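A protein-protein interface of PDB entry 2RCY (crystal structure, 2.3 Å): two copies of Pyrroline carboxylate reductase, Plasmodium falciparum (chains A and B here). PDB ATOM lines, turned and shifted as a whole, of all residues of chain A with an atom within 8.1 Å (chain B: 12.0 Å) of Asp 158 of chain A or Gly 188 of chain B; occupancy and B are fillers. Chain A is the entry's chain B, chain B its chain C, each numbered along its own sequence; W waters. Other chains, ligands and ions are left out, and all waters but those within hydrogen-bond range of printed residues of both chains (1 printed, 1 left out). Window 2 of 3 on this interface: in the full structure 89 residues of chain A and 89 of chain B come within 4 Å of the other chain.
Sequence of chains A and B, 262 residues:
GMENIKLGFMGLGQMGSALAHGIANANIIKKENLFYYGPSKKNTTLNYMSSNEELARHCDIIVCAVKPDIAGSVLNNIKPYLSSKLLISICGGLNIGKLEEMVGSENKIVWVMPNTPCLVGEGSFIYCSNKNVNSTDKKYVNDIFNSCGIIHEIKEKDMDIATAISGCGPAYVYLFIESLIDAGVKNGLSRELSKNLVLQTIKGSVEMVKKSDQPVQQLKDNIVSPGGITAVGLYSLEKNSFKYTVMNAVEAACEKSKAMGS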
ATOM      1  N   TRP A 111       9.515  37.363   0.848  1.00  0.00           N
ATOM      2  CA  TRP A 111      10.567  36.354   0.821  1.00  0.00           C
ATOM      3  C   TRP A 111      10.019  35.002   1.278  1.00  0.00           C
ATOM      4  O   TRP A 111       9.757  34.797   2.465  1.00  0.00           O
ATOM      5  CB  TRP A 111      11.753  36.803   1.685  1.00  0.00           C
ATOM      6  CG  TRP A 111      12.936  35.866   1.691  1.00  0.00           C
ATOM      7  CD1 TRP A 111      13.348  35.048   0.675  1.00  0.00           C
ATOM      8  CD2 TRP A 111      13.879  35.684   2.756  1.00  0.00           C
ATOM      9  NE1 TRP A 111      14.472  34.355   1.049  1.00  0.00           N
ATOM     10  CE2 TRP A 111      14.823  34.728   2.320  1.00  0.00           C
ATOM     11  CE3 TRP A 111      14.011  36.230   4.040  1.00  0.00           C
ATOM     12  CZ2 TRP A 111      15.888  34.305   3.122  1.00  0.00           C
ATOM     13  CZ3 TRP A 111      15.072  35.809   4.837  1.00  0.00           C
ATOM     14  CH2 TRP A 111      15.995  34.856   4.374  1.00  0.00           C
ATOM     15  N   ILE A 126       7.838  28.882   4.442  1.00  0.00           N
ATOM     16  CA  ILE A 126       7.811  30.002   5.380  1.00  0.00           C
ATOM     17  C   ILE A 126       8.032  31.298   4.615  1.00  0.00           C
ATOM     18  O   ILE A 126       8.798  31.329   3.651  1.00  0.00           O
ATOM     19  CB  ILE A 126       8.843  29.875   6.548  1.00  0.00           C
ATOM     20  CG1 ILE A 126      10.284  29.666   6.033  1.00  0.00           C
ATOM     21  CG2 ILE A 126       8.390  28.817   7.566  1.00  0.00           C
ATOM     22  CD1 ILE A 126      10.692  28.218   5.755  1.00  0.00           C
ATOM     23  N   CYS A 128       8.101  35.931   4.868  1.00  0.00           N
ATOM     24  CA  CYS A 128       7.998  37.241   5.495  1.00  0.00           C
ATOM     25  C   CYS A 128       7.850  38.273   4.384  1.00  0.00           C
ATOM     26  O   CYS A 128       8.170  37.992   3.226  1.00  0.00           O
ATOM     27  CB  CYS A 128       9.233  37.533   6.349  1.00  0.00           C
ATOM     28  SG  CYS A 128      10.798  37.478   5.448  1.00  0.00           S
ATOM     29  N   GLU A 153       3.524  32.277   7.892  1.00  0.00           N
ATOM     30  CA  GLU A 153       4.113  33.609   7.981  1.00  0.00           C
ATOM     31  C   GLU A 153       4.910  33.719   9.271  1.00  0.00           C
ATOM     32  O   GLU A 153       4.379  33.500  10.363  1.00  0.00           O
ATOM     33  CB  GLU A 153       3.047  34.706   7.913  1.00  0.00           C
ATOM     34  CG  GLU A 153       3.630  36.119   7.891  1.00  0.00           C
ATOM     35  CD  GLU A 153       2.640  37.175   7.436  1.00  0.00           C
ATOM     36  OE1 GLU A 153       1.427  37.031   7.709  1.00  0.00           O
ATOM     37  OE2 GLU A 153       3.081  38.157   6.806  1.00  0.00           O
ATOM     38  N   ILE A 154       6.190  34.049   9.136  1.00  0.00           N
ATOM     39  CA  ILE A 154       7.081  34.173  10.288  1.00  0.00           C
ATOM     40  C   ILE A 154       7.873  35.482  10.251  1.00  0.00           C
ATOM     41  O   ILE A 154       7.871  36.190   9.241  1.00  0.00           O
ATOM     42  CB  ILE A 154       8.051  32.959  10.412  1.00  0.00           C
ATOM     43  CG1 ILE A 154       8.988  32.873   9.202  1.00  0.00           C
ATOM     44  CG2 ILE A 154       7.270  31.651  10.603  1.00  0.00           C
ATOM     45  CD1 ILE A 154      10.234  32.041   9.447  1.00  0.00           C
ATOM     46  N   LYS A 155       8.539  35.795  11.362  1.00  0.00           N
ATOM     47  CA  LYS A 155       9.431  36.949  11.444  1.00  0.00           C
ATOM     48  C   LYS A 155      10.620  36.786  10.499  1.00  0.00           C
ATOM     49  O   LYS A 155      11.042  35.662  10.209  1.00  0.00           O
ATOM     50  CB  LYS A 155       9.939  37.135  12.876  1.00  0.00           C
ATOM     51  CG  LYS A 155       8.876  37.537  13.883  1.00  0.00           C
ATOM     52  CD  LYS A 155       9.447  37.537  15.289  1.00  0.00           C
ATOM     53  CE  LYS A 155       8.391  37.882  16.323  1.00  0.00           C
ATOM     54  NZ  LYS A 155       8.985  37.998  17.684  1.00  0.00           N
ATOM     55  N   GLU A 156      11.152  37.910  10.024  1.00  0.00           N
ATOM     56  CA  GLU A 156      12.304  37.917   9.123  1.00  0.00           C
ATOM     57  C   GLU A 156      13.553  37.356   9.803  1.00  0.00           C
ATOM     58  O   GLU A 156      14.384  36.714   9.155  1.00  0.00           O
ATOM     59  CB  GLU A 156      12.575  39.333   8.611  1.00  0.00           C
ATOM     60  CG  GLU A 156      13.499  39.395   7.400  1.00  0.00           C
ATOM     61  CD  GLU A 156      14.087  40.774   7.165  1.00  0.00           C
ATOM     62  OE1 GLU A 156      15.224  40.850   6.655  1.00  0.00           O
ATOM     63  OE2 GLU A 156      13.422  41.782   7.486  1.00  0.00           O
ATOM     64  N   LYS A 157      13.671  37.603  11.107  1.00  0.00           N
ATOM     65  CA  LYS A 157      14.790  37.102  11.908  1.00  0.00           C
ATOM     66  C   LYS A 157      14.769  35.577  12.077  1.00  0.00           C
ATOM     67  O   LYS A 157      15.805  34.964  12.336  1.00  0.00           O
ATOM     68  CB  LYS A 157      14.832  37.794  13.280  1.00  0.00           C
ATOM     69  CG  LYS A 157      13.596  37.566  14.160  1.00  0.00           C
ATOM     70  CD  LYS A 157      13.775  38.130  15.571  1.00  0.00           C
ATOM     71  CE  LYS A 157      14.585  37.193  16.474  1.00  0.00           C
ATOM     72  NZ  LYS A 157      13.840  35.948  16.838  1.00  0.00           N
ATOM     73  N   ASP A 158      13.591  34.979  11.923  1.00  0.00           N
ATOM     74  CA  ASP A 158      13.411  33.538  12.097  1.00  0.00           C
ATOM     75  C   ASP A 158      13.571  32.753  10.793  1.00  0.00           C
ATOM     76  O   ASP A 158      13.542  31.521  10.799  1.00  0.00           O
ATOM     77  CB  ASP A 158      12.039  33.247  12.717  1.00  0.00           C
ATOM     78  CG  ASP A 158      11.943  33.683  14.172  1.00  0.00           C
ATOM     79  OD1 ASP A 158      12.993  33.849  14.832  1.00  0.00           O
ATOM     80  OD2 ASP A 158      10.805  33.849  14.660  1.00  0.00           O
ATOM     81  N   MET A 159      13.749  33.473   9.687  1.00  0.00           N
ATOM     82  CA  MET A 159      13.795  32.868   8.350  1.00  0.00           C
ATOM     83  C   MET A 159      14.997  31.956   8.132  1.00  0.00           C
ATOM     84  O   MET A 159      14.903  30.968   7.404  1.00  0.00           O
ATOM     85  CB  MET A 159      13.767  33.949   7.268  1.00  0.00           C
ATOM     86  CG  MET A 159      12.408  34.599   7.046  1.00  0.00           C
ATOM     87  SD  MET A 159      11.113  33.435   6.163  1.00  0.00           S
ATOM     88  CE  MET A 159      12.021  33.144   4.462  1.00  0.00           C
ATOM     89  N   ASP A 160      16.118  32.294   8.764  1.00  0.00           N
ATOM     90  CA  ASP A 160      17.369  31.554   8.597  1.00  0.00           C
ATOM     91  C   ASP A 160      17.317  30.144   9.193  1.00  0.00           C
ATOM     92  O   ASP A 160      17.707  29.177   8.536  1.00  0.00           O
ATOM     93  CB  ASP A 160      18.541  32.351   9.181  1.00  0.00           C
ATOM     94  CG  ASP A 160      18.742  33.686   8.482  1.00  0.00           C
ATOM     95  OD1 ASP A 160      19.157  33.694   7.305  1.00  0.00           O
ATOM     96  OD2 ASP A 160      18.490  34.731   9.117  1.00  0.00           O
ATOM     97  N   ILE A 161      16.831  30.038  10.430  1.00  0.00           N
ATOM     98  CA  ILE A 161      16.651  28.743  11.093  1.00  0.00           C
ATOM     99  C   ILE A 161      15.514  27.937  10.461  1.00  0.00           C
ATOM    100  O   ILE A 161      15.583  26.706  10.384  1.00  0.00           O
ATOM    101  CB  ILE A 161      16.465  28.891  12.645  1.00  0.00           C
ATOM    102  CG1 ILE A 161      16.162  27.543  13.313  1.00  0.00           C
ATOM    103  CG2 ILE A 161      15.386  29.913  12.989  1.00  0.00           C
ATOM    104  CD1 ILE A 161      17.326  26.581  13.337  1.00  0.00           C
ATOM    105  N   ALA A 162      14.483  28.638   9.996  1.00  0.00           N
ATOM    106  CA  ALA A 162      13.369  28.010   9.296  1.00  0.00           C
ATOM    107  C   ALA A 162      13.799  27.464   7.935  1.00  0.00           C
ATOM    108  O   ALA A 162      13.317  26.417   7.511  1.00  0.00           O
ATOM    109  CB  ALA A 162      12.217  28.982   9.148  1.00  0.00           C
ATOM    110  N   THR A 163      14.704  28.175   7.259  1.00  0.00           N
ATOM    111  CA  THR A 163      15.324  27.677   6.027  1.00  0.00           C
ATOM    112  C   THR A 163      16.098  26.395   6.326  1.00  0.00           C
ATOM    113  O   THR A 163      15.974  25.405   5.604  1.00  0.00           O
ATOM    114  CB  THR A 163      16.280  28.723   5.392  1.00  0.00           C
ATOM    115  OG1 THR A 163      15.560  29.926   5.097  1.00  0.00           O
ATOM    116  CG2 THR A 163      16.910  28.189   4.104  1.00  0.00           C
ATOM    117  N   ALA A 164      16.878  26.426   7.405  1.00  0.00           N
ATOM    118  CA  ALA A 164      17.707  25.297   7.825  1.00  0.00           C
ATOM    119  C   ALA A 164      16.897  24.029   8.112  1.00  0.00           C
ATOM    120  O   ALA A 164      17.368  22.921   7.857  1.00  0.00           O
ATOM    121  CB  ALA A 164      18.541  25.683   9.036  1.00  0.00           C
ATOM    122  N   ILE A 165      15.680  24.200   8.623  1.00  0.00           N
ATOM    123  CA  ILE A 165      14.795  23.075   8.932  1.00  0.00           C
ATOM    124  C   ILE A 165      13.875  22.714   7.766  1.00  0.00           C
ATOM    125  O   ILE A 165      13.817  21.558   7.357  1.00  0.00           O
ATOM    126  CB  ILE A 165      13.945  23.340  10.200  1.00  0.00           C
ATOM    127  CG1 ILE A 165      14.850  23.534  11.421  1.00  0.00           C
ATOM    128  CG2 ILE A 165      12.967  22.192  10.445  1.00  0.00           C
ATOM    129  CD1 ILE A 165      14.140  24.068  12.640  1.00  0.00           C
ATOM    130  N   CYS A 254      21.968  27.077   9.488  1.00  0.00           N
ATOM    131  CA  CYS A 254      21.458  28.364   9.964  1.00  0.00           C
ATOM    132  C   CYS A 254      22.535  29.451   9.945  1.00  0.00           C
ATOM    133  O   CYS A 254      22.260  30.592   9.566  1.00  0.00           O
ATOM    134  CB  CYS A 254      20.867  28.219  11.368  1.00  0.00           C
ATOM    135  SG  CYS A 254      20.065  29.704  12.003  1.00  0.00           S
ATOM    136  N   SER A 257      23.113  30.500   6.269  1.00  0.00           N
ATOM    137  CA  SER A 257      22.010  31.351   5.824  1.00  0.00           C
ATOM    138  C   SER A 257      22.204  32.803   6.272  1.00  0.00           C
ATOM    139  O   SER A 257      22.011  33.731   5.485  1.00  0.00           O
ATOM    140  CB  SER A 257      20.674  30.806   6.337  1.00  0.00           C
ATOM    141  OG  SER A 257      19.582  31.508   5.773  1.00  0.00           O
ATOM    142  N   LYS A 258      22.600  32.983   7.532  1.00  0.00           N
ATOM    143  CA  LYS A 258      22.849  34.309   8.097  1.00  0.00           C
ATOM    144  C   LYS A 258      24.070  34.979   7.474  1.00  0.00           C
ATOM    145  O   LYS A 258      24.037  36.174   7.174  1.00  0.00           O
ATOM    146  CB  LYS A 258      23.004  34.234   9.620  1.00  0.00           C
ATOM    147  CG  LYS A 258      21.724  33.876  10.350  1.00  0.00           C
ATOM    148  CD  LYS A 258      21.864  34.031  11.852  1.00  0.00           C
ATOM    149  CE  LYS A 258      20.546  33.717  12.544  1.00  0.00           C
ATOM    150  NZ  LYS A 258      20.607  33.942  14.015  1.00  0.00           N
ATOM    151  N   SER B 179      14.986  15.949  17.807  1.00  0.00           N
ATOM    152  CA  SER B 179      16.259  16.652  17.638  1.00  0.00           C
ATOM    153  C   SER B 179      16.138  17.855  16.706  1.00  0.00           C
ATOM    154  O   SER B 179      16.789  18.880  16.920  1.00  0.00           O
ATOM    155  CB  SER B 179      17.337  15.694  17.122  1.00  0.00           C
ATOM    156  OG  SER B 179      17.444  14.547  17.949  1.00  0.00           O
ATOM    157  N   LEU B 180      15.304  17.722  15.675  1.00  0.00           N
ATOM    158  CA  LEU B 180      15.076  18.797  14.709  1.00  0.00           C
ATOM    159  C   LEU B 180      14.317  19.964  15.340  1.00  0.00           C
ATOM    160  O   LEU B 180      14.605  21.129  15.047  1.00  0.00           O
ATOM    161  CB  LEU B 180      14.342  18.273  13.467  1.00  0.00           C
ATOM    162  CG  LEU B 180      15.091  17.367  12.477  1.00  0.00           C
ATOM    163  CD1 LEU B 180      14.111  16.625  11.584  1.00  0.00           C
ATOM    164  CD2 LEU B 180      16.092  18.144  11.627  1.00  0.00           C
ATOM    165  N   ILE B 181      13.360  19.645  16.212  1.00  0.00           N
ATOM    166  CA  ILE B 181      12.617  20.657  16.967  1.00  0.00           C
ATOM    167  C   ILE B 181      13.540  21.399  17.939  1.00  0.00           C
ATOM    168  O   ILE B 181      13.535  22.631  17.981  1.00  0.00           O
ATOM    169  CB  ILE B 181      11.399  20.046  17.714  1.00  0.00           C
ATOM    170  CG1 ILE B 181      10.388  19.482  16.712  1.00  0.00           C
ATOM    171  CG2 ILE B 181      10.727  21.090  18.613  1.00  0.00           C
ATOM    172  CD1 ILE B 181       9.419  18.462  17.295  1.00  0.00           C
ATOM    173  N   ASP B 182      14.333  20.642  18.698  1.00  0.00           N
ATOM    174  CA  ASP B 182      15.316  21.205  19.636  1.00  0.00           C
ATOM    175  C   ASP B 182      16.293  22.172  18.967  1.00  0.00           C
ATOM    176  O   ASP B 182      16.706  23.161  19.573  1.00  0.00           O
ATOM    177  CB  ASP B 182      16.098  20.087  20.333  1.00  0.00           C
ATOM    178  CG  ASP B 182      15.285  19.375  21.396  1.00  0.00           C
ATOM    179  OD1 ASP B 182      14.044  19.535  21.428  1.00  0.00           O
ATOM    180  OD2 ASP B 182      15.891  18.644  22.207  1.00  0.00           O
ATOM    181  N   ALA B 183      16.658  21.871  17.722  1.00  0.00           N
ATOM    182  CA  ALA B 183      17.543  22.722  16.934  1.00  0.00           C
ATOM    183  C   ALA B 183      16.851  24.026  16.548  1.00  0.00           C
ATOM    184  O   ALA B 183      17.471  25.090  16.556  1.00  0.00           O
ATOM    185  CB  ALA B 183      18.019  21.985  15.695  1.00  0.00           C
ATOM    186  N   GLY B 184      15.564  23.931  16.212  1.00  0.00           N
ATOM    187  CA  GLY B 184      14.745  25.099  15.908  1.00  0.00           C
ATOM    188  C   GLY B 184      14.533  25.974  17.126  1.00  0.00           C
ATOM    189  O   GLY B 184      14.680  27.197  17.053  1.00  0.00           O
ATOM    190  N   VAL B 185      14.200  25.337  18.246  1.00  0.00           N
ATOM    191  CA  VAL B 185      13.976  26.033  19.511  1.00  0.00           C
ATOM    192  C   VAL B 185      15.242  26.756  19.971  1.00  0.00           C
ATOM    193  O   VAL B 185      15.176  27.911  20.393  1.00  0.00           O
ATOM    194  CB  VAL B 185      13.446  25.077  20.617  1.00  0.00           C
ATOM    195  CG1 VAL B 185      13.282  25.813  21.945  1.00  0.00           C
ATOM    196  CG2 VAL B 185      12.119  24.459  20.196  1.00  0.00           C
ATOM    197  N   LYS B 186      16.388  26.082  19.864  1.00  0.00           N
ATOM    198  CA  LYS B 186      17.671  26.667  20.256  1.00  0.00           C
ATOM    199  C   LYS B 186      17.983  27.951  19.486  1.00  0.00           C
ATOM    200  O   LYS B 186      18.573  28.883  20.035  1.00  0.00           O
ATOM    201  CB  LYS B 186      18.814  25.657  20.079  1.00  0.00           C
ATOM    202  CG  LYS B 186      20.157  26.149  20.605  1.00  0.00           C
ATOM    203  CD  LYS B 186      21.268  25.149  20.379  1.00  0.00           C
ATOM    204  CE  LYS B 186      22.589  25.679  20.915  1.00  0.00           C
ATOM    205  NZ  LYS B 186      23.199  26.716  20.045  1.00  0.00           N
ATOM    206  N   ASN B 187      17.576  27.992  18.220  1.00  0.00           N
ATOM    207  CA  ASN B 187      17.903  29.109  17.345  1.00  0.00           C
ATOM    208  C   ASN B 187      16.748  30.083  17.090  1.00  0.00           C
ATOM    209  O   ASN B 187      16.706  30.748  16.051  1.00  0.00           O
ATOM    210  CB  ASN B 187      18.498  28.589  16.036  1.00  0.00           C
ATOM    211  CG  ASN B 187      19.828  27.895  16.241  1.00  0.00           C
ATOM    212  OD1 ASN B 187      20.849  28.544  16.454  1.00  0.00           O
ATOM    213  ND2 ASN B 187      19.823  26.567  16.174  1.00  0.00           N
ATOM    214  N   GLY B 188      15.813  30.160  18.036  1.00  0.00           N
ATOM    215  CA  GLY B 188      14.803  31.219  18.029  1.00  0.00           C
ATOM    216  C   GLY B 188      13.365  30.846  17.725  1.00  0.00           C
ATOM    217  O   GLY B 188      12.452  31.608  18.050  1.00  0.00           O
ATOM    218  N   LEU B 189      13.154  29.692  17.095  1.00  0.00           N
ATOM    219  CA  LEU B 189      11.803  29.246  16.740  1.00  0.00           C
ATOM    220  C   LEU B 189      11.029  28.739  17.951  1.00  0.00           C
ATOM    221  O   LEU B 189      11.620  28.253  18.917  1.00  0.00           O
ATOM    222  CB  LEU B 189      11.839  28.157  15.661  1.00  0.00           C
ATOM    223  CG  LEU B 189      12.340  28.471  14.248  1.00  0.00           C
ATOM    224  CD1 LEU B 189      12.175  27.253  13.352  1.00  0.00           C
ATOM    225  CD2 LEU B 189      11.636  29.679  13.636  1.00  0.00           C
ATOM    226  N   SER B 190       9.705  28.864  17.894  1.00  0.00           N
ATOM    227  CA  SER B 190       8.840  28.315  18.934  1.00  0.00           C
ATOM    228  C   SER B 190       8.747  26.802  18.770  1.00  0.00           C
ATOM    229  O   SER B 190       8.903  26.282  17.662  1.00  0.00           O
ATOM    230  CB  SER B 190       7.447  28.954  18.883  1.00  0.00           C
ATOM    231  OG  SER B 190       6.720  28.532  17.740  1.00  0.00           O
ATOM    232  N   ARG B 191       8.503  26.102  19.875  1.00  0.00           N
ATOM    233  CA  ARG B 191       8.381  24.645  19.865  1.00  0.00           C
ATOM    234  C   ARG B 191       7.258  24.168  18.937  1.00  0.00           C
ATOM    235  O   ARG B 191       7.413  23.167  18.235  1.00  0.00           O
ATOM    236  CB  ARG B 191       8.193  24.121  21.296  1.00  0.00           C
ATOM    237  CG  ARG B 191       8.135  22.604  21.431  1.00  0.00           C
ATOM    238  CD  ARG B 191       8.672  22.133  22.777  1.00  0.00           C
ATOM    239  NE  ARG B 191      10.091  21.782  22.700  1.00  0.00           N
ATOM    240  CZ  ARG B 191      11.072  22.409  23.345  1.00  0.00           C
ATOM    241  NH1 ARG B 191      12.323  21.999  23.193  1.00  0.00           N
ATOM    242  NH2 ARG B 191      10.814  23.437  24.146  1.00  0.00           N
ATOM    243  N   GLU B 192       6.147  24.906  18.923  1.00  0.00           N
ATOM    244  CA  GLU B 192       4.989  24.579  18.086  1.00  0.00           C
ATOM    245  C   GLU B 192       5.290  24.721  16.593  1.00  0.00           C
ATOM    246  O   GLU B 192       4.951  23.840  15.804  1.00  0.00           O
ATOM    247  CB  GLU B 192       3.786  25.446  18.476  1.00  0.00           C
ATOM    248  CG  GLU B 192       2.457  25.017  17.857  1.00  0.00           C
ATOM    249  CD  GLU B 192       1.312  25.952  18.218  1.00  0.00           C
ATOM    250  OE1 GLU B 192       0.867  25.937  19.387  1.00  0.00           O
ATOM    251  OE2 GLU B 192       0.851  26.699  17.328  1.00  0.00           O
ATOM    252  N   LEU B 193       5.926  25.831  16.217  1.00  0.00           N
ATOM    253  CA  LEU B 193       6.283  26.098  14.823  1.00  0.00           C
ATOM    254  C   LEU B 193       7.356  25.137  14.316  1.00  0.00           C
ATOM    255  O   LEU B 193       7.258  24.624  13.197  1.00  0.00           O
ATOM    256  CB  LEU B 193       6.741  27.552  14.654  1.00  0.00           C
ATOM    257  CG  LEU B 193       7.306  28.007  13.305  1.00  0.00           C
ATOM    258  CD1 LEU B 193       6.235  28.021  12.224  1.00  0.00           C
ATOM    259  CD2 LEU B 193       7.943  29.375  13.446  1.00  0.00           C
ATOM    260  N   SER B 194       8.376  24.904  15.141  1.00  0.00           N
ATOM    261  CA  SER B 194       9.436  23.951  14.825  1.00  0.00           C
ATOM    262  C   SER B 194       8.837  22.589  14.493  1.00  0.00           C
ATOM    263  O   SER B 194       9.151  22.010  13.456  1.00  0.00           O
ATOM    264  CB  SER B 194      10.424  23.828  15.985  1.00  0.00           C
ATOM    265  OG  SER B 194      10.949  25.092  16.346  1.00  0.00           O
ATOM    266  N   LYS B 195       7.958  22.105  15.370  1.00  0.00           N
ATOM    267  CA  LYS B 195       7.248  20.839  15.178  1.00  0.00           C
ATOM    268  C   LYS B 195       6.508  20.792  13.840  1.00  0.00           C
ATOM    269  O   LYS B 195       6.668  19.837  13.077  1.00  0.00           O
ATOM    270  CB  LYS B 195       6.278  20.597  16.339  1.00  0.00           C
ATOM    271  CG  LYS B 195       5.652  19.205  16.372  1.00  0.00           C
ATOM    272  CD  LYS B 195       4.819  18.985  17.632  1.00  0.00           C
ATOM    273  CE  LYS B 195       3.454  19.663  17.548  1.00  0.00           C
ATOM    274  NZ  LYS B 195       2.627  19.403  18.764  1.00  0.00           N
ATOM    275  N   LEU B 197       6.879  22.639  11.078  1.00  0.00           N
ATOM    276  CA  LEU B 197       7.829  22.665   9.969  1.00  0.00           C
ATOM    277  C   LEU B 197       8.537  21.322   9.790  1.00  0.00           C
ATOM    278  O   LEU B 197       8.702  20.852   8.664  1.00  0.00           O
ATOM    279  CB  LEU B 197       8.852  23.790  10.166  1.00  0.00           C
ATOM    280  CG  LEU B 197       8.690  25.109   9.396  1.00  0.00           C
ATOM    281  CD1 LEU B 197       7.264  25.647   9.406  1.00  0.00           C
ATOM    282  CD2 LEU B 197       9.653  26.149   9.941  1.00  0.00           C
ATOM    283  N   VAL B 198       8.936  20.709  10.905  1.00  0.00           N
ATOM    284  CA  VAL B 198       9.604  19.404  10.897  1.00  0.00           C
ATOM    285  C   VAL B 198       8.710  18.318  10.292  1.00  0.00           C
ATOM    286  O   VAL B 198       9.106  17.652   9.335  1.00  0.00           O
ATOM    287  CB  VAL B 198      10.078  18.996  12.322  1.00  0.00           C
ATOM    288  CG1 VAL B 198      10.507  17.531  12.371  1.00  0.00           C
ATOM    289  CG2 VAL B 198      11.213  19.890  12.780  1.00  0.00           C
ATOM    290  N   ILE B 229      23.243  26.637   1.197  1.00  0.00           N
ATOM    291  CA  ILE B 229      23.045  26.399   2.625  1.00  0.00           C
ATOM    292  C   ILE B 229      23.004  24.905   2.958  1.00  0.00           C
ATOM    293  O   ILE B 229      23.605  24.468   3.942  1.00  0.00           O
ATOM    294  CB  ILE B 229      21.744  27.095   3.125  1.00  0.00           C
ATOM    295  CG1 ILE B 229      21.757  28.587   2.770  1.00  0.00           C
ATOM    296  CG2 ILE B 229      21.558  26.907   4.625  1.00  0.00           C
ATOM    297  CD1 ILE B 229      20.378  29.228   2.707  1.00  0.00           C
HETATM  298  O   HOH W   1      18.794  31.809  14.707  1.00  0.00           O
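No position is printed for both chains. Of the 15 pairs that touch across the chains among the printed residues, none has its exchanged pair printed and touching as well.
The side-chain amino group of Lys 157 of chain A lies within salt-bridge range of the side-chain carboxylate of Asp 158 of chain A (3.0 Å). The backbone carbonyl oxygen (O) of Met 159 of chain A sits at hydrogen-bond distance from the side-chain hydroxyl (OG1) of Thr 163 of chain A (2.6 Å). N of Ile 161 of chain A is in hydrogen-bond range of SG of Cys 254 of chain A (3.6 Å). The backbone carbonyl oxygen (O) of Ala 183 of chain B lies within hydrogen-bond range of the side-chain amide nitrogen (ND2) of Asn 187 of chain B, at 2.8 Å. The backbone carbonyl oxygen (O) of Gly 184 of chain B lies within hydrogen-bond range of the backbone NH (N) of Leu 189 of chain B (2.9 Å). The side-chain hydroxyl (OG) of Ser 190 of chain B lies within hydrogen-bond range of the backbone NH (N) of Leu 193 of chain B (3.2 Å).
Of the 20 printed residues of chain B, 10 touch a printed residue of chain A. Printed residues of chain B that touch a printed residue of chain A: Leu 180, Ala 183, Gly 184, Asn 187, Gly 188, Leu 189, Leu 193, Leu 197, Val 198 and Ile 229. Hydrophobic or aromatic side chains of chain B that line the printed part of chain A: Leu 189, Leu 193, Leu 197, Val 198 and Ile 229. Among the printed residues, 15 pairs touch across the chains. Among the printed residues, no Asp or Glu carboxylate lies within 4 Å of a Lys or Arg side-chain nitrogen of the other chain.
Water W1 lies within hydrogen-bond range of O of Asn 187 of chain B (2.7 Å), NZ of Lys 258 of chain A (2.9 Å) and SG of Cys 254 of chain A (3.7 Å).
Ile 126 of chain A touches Leu 197 of chain B. Leu 193 of chain B touches Ile 154 of chain A (CD2 to CG2, 3.7 Å). Asp 158 of chain A touches Leu 189 of chain B (CB to CD2, 3.7 Å). CD1 of Ile 161 of chain A touches O of Ala 183 of chain B, 3.6 Å away. Leu 189 of chain B touches Ile 161 of chain A. CD2 of Leu 197 of chain B touches CB of Ala 162 of chain A, 3.9 Å away. Leu 180 of chain B touches Ile 165 of chain A. Ile 165 of chain A touches Gly 184 of chain B. Leu 189 of chain B touches Ile 165 of chain A. Val 198 of chain B touches Ile 165 of chain A (CG2 to CG2, 3.7 Å).
Ile 154 of chain A touches just one residue of chain B: Leu 193. No residue of chain B comes within 4 Å of Lys 155 of chain A. No residue of chain B comes within 4 Å of Lys 157 of chain A. No residue of chain B comes within 4 Å of Met 159 of chain A. Of chain B, only Leu 197 (3.9 Å) comes within 4 Å of Ala 162 of chain A. Of the printed residues of chain B, Ile 165 of chain A touches Leu 180, Gly 184, Leu 189 and Val 198. Of the printed residues of chain A, Ala 183 of chain B touches Ile 161. Of the printed residues of chain A, Gly 184 of chain B touches Ile 161 (3.8 Å) and Ile 165 (3.5 Å). Lys 186 of chain B touches none of the printed residues of chain A. Of the printed residues of chain A, Asn 187 of chain B touches Ile 161. Of the printed residues of chain A, Gly 188 of chain B touches Asp 158. Ser 194 of chain B touches none of the printed residues of chain A. The nearest printed residue of chain A that does not touch Val 198 of chain B is Ala 162 of chain A (8.0 Å).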
